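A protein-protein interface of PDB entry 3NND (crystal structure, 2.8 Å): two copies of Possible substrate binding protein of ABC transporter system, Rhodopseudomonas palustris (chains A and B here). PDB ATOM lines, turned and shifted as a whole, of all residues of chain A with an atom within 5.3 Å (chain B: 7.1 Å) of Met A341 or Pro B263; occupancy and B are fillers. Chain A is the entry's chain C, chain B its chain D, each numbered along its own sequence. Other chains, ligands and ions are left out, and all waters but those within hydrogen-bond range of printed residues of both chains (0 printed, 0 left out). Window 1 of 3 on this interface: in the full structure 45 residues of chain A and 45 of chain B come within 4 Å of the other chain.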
ATOM      1  N   GLN A 339     -22.697 -33.273  -6.293  1.00  0.00           N
ATOM      2  CA  GLN A 339     -22.996 -32.126  -7.121  1.00  0.00           C
ATOM      3  C   GLN A 339     -23.102 -30.885  -6.212  1.00  0.00           C
ATOM      4  O   GLN A 339     -23.895 -30.865  -5.261  1.00  0.00           O
ATOM      5  CB  GLN A 339     -24.316 -32.368  -7.862  1.00  0.00           C
ATOM      6  CG  GLN A 339     -24.551 -31.472  -9.054  1.00  0.00           C
ATOM      7  CD  GLN A 339     -23.675 -31.850 -10.211  1.00  0.00           C
ATOM      8  OE1 GLN A 339     -23.670 -33.000 -10.633  1.00  0.00           O
ATOM      9  NE2 GLN A 339     -22.917 -30.888 -10.729  1.00  0.00           N
ATOM     10  N   SER A 340     -22.284 -29.870  -6.488  1.00  0.00           N
ATOM     11  CA  SER A 340     -22.355 -28.598  -5.770  1.00  0.00           C
ATOM     12  C   SER A 340     -23.422 -27.715  -6.389  1.00  0.00           C
ATOM     13  O   SER A 340     -23.418 -27.494  -7.596  1.00  0.00           O
ATOM     14  CB  SER A 340     -21.027 -27.871  -5.826  1.00  0.00           C
ATOM     15  OG  SER A 340     -21.062 -26.740  -4.983  1.00  0.00           O
ATOM     16  N   MET A 341     -24.331 -27.196  -5.571  1.00  0.00           N
ATOM     17  CA  MET A 341     -25.552 -26.621  -6.120  1.00  0.00           C
ATOM     18  C   MET A 341     -26.135 -25.413  -5.400  1.00  0.00           C
ATOM     19  O   MET A 341     -25.917 -25.204  -4.202  1.00  0.00           O
ATOM     20  CB  MET A 341     -26.607 -27.711  -6.234  1.00  0.00           C
ATOM     21  CG  MET A 341     -26.110 -28.855  -7.048  1.00  0.00           C
ATOM     22  SD  MET A 341     -27.447 -29.617  -8.201  1.00  0.00           S
ATOM     23  CE  MET A 341     -28.084 -30.996  -6.972  1.00  0.00           C
ATOM     24  N   TYR A 342     -26.874 -24.615  -6.164  1.00  0.00           N
ATOM     25  CA  TYR A 342     -27.646 -23.527  -5.599  1.00  0.00           C
ATOM     26  C   TYR A 342     -29.082 -23.981  -5.500  1.00  0.00           C
ATOM     27  O   TYR A 342     -29.490 -24.912  -6.185  1.00  0.00           O
ATOM     28  CB  TYR A 342     -27.546 -22.271  -6.455  1.00  0.00           C
ATOM     29  CG  TYR A 342     -26.295 -21.486  -6.197  1.00  0.00           C
ATOM     30  CD1 TYR A 342     -26.012 -20.993  -4.925  1.00  0.00           C
ATOM     31  CD2 TYR A 342     -25.391 -21.236  -7.217  1.00  0.00           C
ATOM     32  CE1 TYR A 342     -24.864 -20.270  -4.681  1.00  0.00           C
ATOM     33  CE2 TYR A 342     -24.240 -20.515  -6.986  1.00  0.00           C
ATOM     34  CZ  TYR A 342     -23.976 -20.036  -5.720  1.00  0.00           C
ATOM     35  OH  TYR A 342     -22.814 -19.327  -5.507  1.00  0.00           O
ATOM     36  N   HIS A 343     -29.846 -23.325  -4.642  1.00  0.00           N
ATOM     37  CA  HIS A 343     -31.239 -23.687  -4.464  1.00  0.00           C
ATOM     38  C   HIS A 343     -32.187 -22.578  -4.895  1.00  0.00           C
ATOM     39  O   HIS A 343     -32.065 -21.429  -4.472  1.00  0.00           O
ATOM     40  CB  HIS A 343     -31.475 -24.117  -3.025  1.00  0.00           C
ATOM     41  CG  HIS A 343     -30.571 -25.228  -2.598  1.00  0.00           C
ATOM     42  ND1 HIS A 343     -30.790 -26.540  -2.957  1.00  0.00           N
ATOM     43  CD2 HIS A 343     -29.425 -25.220  -1.880  1.00  0.00           C
ATOM     44  CE1 HIS A 343     -29.827 -27.295  -2.459  1.00  0.00           C
ATOM     45  NE2 HIS A 343     -28.988 -26.520  -1.798  1.00  0.00           N
ATOM     46  N   ASP B 261     -33.101 -27.651  -7.593  1.00  0.00           N
ATOM     47  CA  ASP B 261     -31.672 -27.394  -7.417  1.00  0.00           C
ATOM     48  C   ASP B 261     -30.947 -27.151  -8.737  1.00  0.00           C
ATOM     49  O   ASP B 261     -31.306 -27.715  -9.769  1.00  0.00           O
ATOM     50  CB  ASP B 261     -31.000 -28.541  -6.662  1.00  0.00           C
ATOM     51  CG  ASP B 261     -31.360 -28.565  -5.193  1.00  0.00           C
ATOM     52  OD1 ASP B 261     -32.032 -27.627  -4.709  1.00  0.00           O
ATOM     53  OD2 ASP B 261     -30.968 -29.538  -4.518  1.00  0.00           O
ATOM     54  N   ILE B 262     -29.921 -26.308  -8.695  1.00  0.00           N
ATOM     55  CA  ILE B 262     -29.153 -25.993  -9.890  1.00  0.00           C
ATOM     56  C   ILE B 262     -27.675 -26.155  -9.635  1.00  0.00           C
ATOM     57  O   ILE B 262     -27.157 -25.683  -8.620  1.00  0.00           O
ATOM     58  CB  ILE B 262     -29.395 -24.549 -10.384  1.00  0.00           C
ATOM     59  CG1 ILE B 262     -30.858 -24.347 -10.790  1.00  0.00           C
ATOM     60  CG2 ILE B 262     -28.480 -24.240 -11.550  1.00  0.00           C
ATOM     61  CD1 ILE B 262     -31.297 -25.216 -11.967  1.00  0.00           C
ATOM     62  N   PRO B 263     -26.994 -26.840 -10.562  1.00  0.00           N
ATOM     63  CA  PRO B 263     -25.538 -26.959 -10.609  1.00  0.00           C
ATOM     64  C   PRO B 263     -24.903 -25.584 -10.666  1.00  0.00           C
ATOM     65  O   PRO B 263     -25.142 -24.863 -11.631  1.00  0.00           O
ATOM     66  CB  PRO B 263     -25.297 -27.685 -11.931  1.00  0.00           C
ATOM     67  CG  PRO B 263     -26.520 -28.482 -12.137  1.00  0.00           C
ATOM     68  CD  PRO B 263     -27.644 -27.649 -11.605  1.00  0.00           C
ATOM     69  N   LYS B 264     -24.112 -25.241  -9.651  1.00  0.00           N
ATOM     70  CA  LYS B 264     -23.434 -23.952  -9.573  1.00  0.00           C
ATOM     71  C   LYS B 264     -22.632 -23.657 -10.828  1.00  0.00           C
ATOM     72  O   LYS B 264     -21.978 -24.538 -11.377  1.00  0.00           O
ATOM     73  CB  LYS B 264     -22.493 -23.908  -8.364  1.00  0.00           C
ATOM     74  CG  LYS B 264     -23.177 -23.808  -6.997  1.00  0.00           C
ATOM     75  CD  LYS B 264     -22.143 -23.724  -5.893  1.00  0.00           C
ATOM     76  CE  LYS B 264     -22.666 -23.040  -4.652  1.00  0.00           C
ATOM     77  NZ  LYS B 264     -21.518 -22.465  -3.873  1.00  0.00           N
ATOM     78  N   ASN B 265     -22.679 -22.409 -11.276  1.00  0.00           N
ATOM     79  CA  ASN B 265     -21.790 -21.948 -12.334  1.00  0.00           C
ATOM     80  C   ASN B 265     -21.406 -20.475 -12.133  1.00  0.00           C
ATOM     81  O   ASN B 265     -21.883 -19.829 -11.207  1.00  0.00           O
ATOM     82  CB  ASN B 265     -22.381 -22.247 -13.718  1.00  0.00           C
ATOM     83  CG  ASN B 265     -23.644 -21.475 -14.000  1.00  0.00           C
ATOM     84  OD1 ASN B 265     -23.781 -20.328 -13.594  1.00  0.00           O
ATOM     85  ND2 ASN B 265     -24.569 -22.092 -14.721  1.00  0.00           N
ATOM     86  N   PRO B 266     -20.494 -19.958 -12.960  1.00  0.00           N
ATOM     87  CA  PRO B 266     -20.110 -18.553 -12.797  1.00  0.00           C
ATOM     88  C   PRO B 266     -21.281 -17.570 -12.854  1.00  0.00           C
ATOM     89  O   PRO B 266     -21.206 -16.527 -12.210  1.00  0.00           O
ATOM     90  CB  PRO B 266     -19.148 -18.327 -13.960  1.00  0.00           C
ATOM     91  CG  PRO B 266     -18.499 -19.656 -14.128  1.00  0.00           C
ATOM     92  CD  PRO B 266     -19.570 -20.673 -13.857  1.00  0.00           C
ATOM     93  N   ASN B 268     -24.863 -18.403 -12.171  1.00  0.00           N
ATOM     94  CA  ASN B 268     -25.444 -18.755 -10.882  1.00  0.00           C
ATOM     95  C   ASN B 268     -24.896 -17.861  -9.786  1.00  0.00           C
ATOM     96  O   ASN B 268     -25.603 -17.023  -9.231  1.00  0.00           O
ATOM     97  CB  ASN B 268     -25.027 -20.180 -10.513  1.00  0.00           C
ATOM     98  CG  ASN B 268     -26.031 -21.209 -10.934  1.00  0.00           C
ATOM     99  OD1 ASN B 268     -27.234 -21.022 -10.776  1.00  0.00           O
ATOM    100  ND2 ASN B 268     -25.545 -22.318 -11.464  1.00  0.00           N
ATOM    101  N   PRO B 324     -28.170 -18.529 -16.246  1.00  0.00           N
ATOM    102  CA  PRO B 324     -28.036 -18.895 -14.837  1.00  0.00           C
ATOM    103  C   PRO B 324     -28.177 -20.385 -14.576  1.00  0.00           C
ATOM    104  O   PRO B 324     -27.862 -20.820 -13.476  1.00  0.00           O
ATOM    105  CB  PRO B 324     -29.198 -18.157 -14.186  1.00  0.00           C
ATOM    106  CG  PRO B 324     -29.390 -16.963 -15.038  1.00  0.00           C
ATOM    107  CD  PRO B 324     -29.083 -17.388 -16.432  1.00  0.00           C
ATOM    108  N   LYS B 325     -28.651 -21.155 -15.551  1.00  0.00           N
ATOM    109  CA  LYS B 325     -28.813 -22.592 -15.340  1.00  0.00           C
ATOM    110  C   LYS B 325     -27.949 -23.426 -16.286  1.00  0.00           C
ATOM    111  O   LYS B 325     -28.115 -24.648 -16.378  1.00  0.00           O
ATOM    112  CB  LYS B 325     -30.293 -22.999 -15.433  1.00  0.00           C
ATOM    113  CG  LYS B 325     -30.770 -23.432 -16.822  1.00  0.00           C
ATOM    114  CD  LYS B 325     -32.293 -23.553 -16.892  1.00  0.00           C
ATOM    115  CE  LYS B 325     -32.964 -22.180 -17.027  1.00  0.00           C
ATOM    116  NZ  LYS B 325     -34.402 -22.214 -16.614  1.00  0.00           N
ATOM    117  N   GLY B 326     -27.018 -22.766 -16.976  1.00  0.00           N
ATOM    118  CA  GLY B 326     -26.126 -23.455 -17.887  1.00  0.00           C
ATOM    119  C   GLY B 326     -26.287 -23.010 -19.331  1.00  0.00           C
ATOM    120  O   GLY B 326     -26.901 -21.980 -19.592  1.00  0.00           O
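The backbone NH (N) of Lys B264 sits at hydrogen-bond distance from the backbone carbonyl oxygen (O) of Ser A340. The backbone NH of Tyr A342 sits at hydrogen-bond distance from the backbone carbonyl oxygen of Ile B262, at 2.7 Å. The side-chain carboxylate (OD1) of Asp B261 lies within hydrogen-bond range of a ring nitrogen (ND1) of His A343 (2.4 Å). SD of Met A341 sits close to N of Pro B263 (3.7 Å).
ND2 of Asn B268 lies within hydrogen-bond range of O of Pro B263, 2.6 Å away. N of Asn B268 is in hydrogen-bond range of OD1 of Asn B265, at 2.6 Å. The backbone carbonyl oxygen (O) of Pro B324 sits close to the side-chain amide oxygen (OD1) of Asn B268.
Pro B263 touches Ser A340. Met A341 touches Asp B261. Ile B262 touches Met A341 (O to CA, 3.1 Å). Met A341 touches Lys B264. CA of Asp B261 touches O of Tyr A342, 3.5 Å away. CD2 of Tyr A342 touches CG of Lys B264, at 3.4 Å. Tyr A342 touches Asn B268.
Gln A339 touches none of the printed residues of chain B. Of the printed residues of chain B, Ser A340 touches Pro B263 (3.7 Å) and Lys B264 (3.1 Å). Of chain B, only Asp B261, Ile B262, Pro B263 and Lys B264 come within 4 Å of Met A341. Of the printed residues of chain B, Tyr A342 touches Asp B261, Ile B262, Lys B264 and Asn B268. Of the printed residues of chain A, Asp B261 touches Met A341, Tyr A342 and His A343. Of the printed residues of chain A, Ile B262 touches Met A341 (3.1 Å) and Tyr A342 (2.7 Å). Pro B263 touches two residues of chain A. Of the printed residues of chain A, Lys B264 touches Ser A340 (3.1 Å), Met A341 (3.7 Å) and Tyr A342 (3.4 Å). Asn B265 touches none of the printed residues of chain A. The nearest printed residue of chain B that does not touch Ser A340 is Ile B262 (4.3 Å).
Of the 10 printed residues of chain B, 5 touch a printed residue of chain A. Hydrophobic or aromatic side chains of chain B that line the printed part of chain A: Pro B263. Of the 5 printed residues of chain A, 4 touch a printed residue of chain B. Hydrophobic or aromatic side chains of chain A within 4 Å of the printed part of chain B: Met A341, Tyr A342 and His A343. Among the printed residues, no Asp or Glu carboxylate lies within 4 Å of a Lys or Arg side-chain nitrogen of the other chain.
No position is printed for both chains. Of the 11 pairs that touch across the chains among the printed residues, none has its exchanged pair printed and touching as well.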
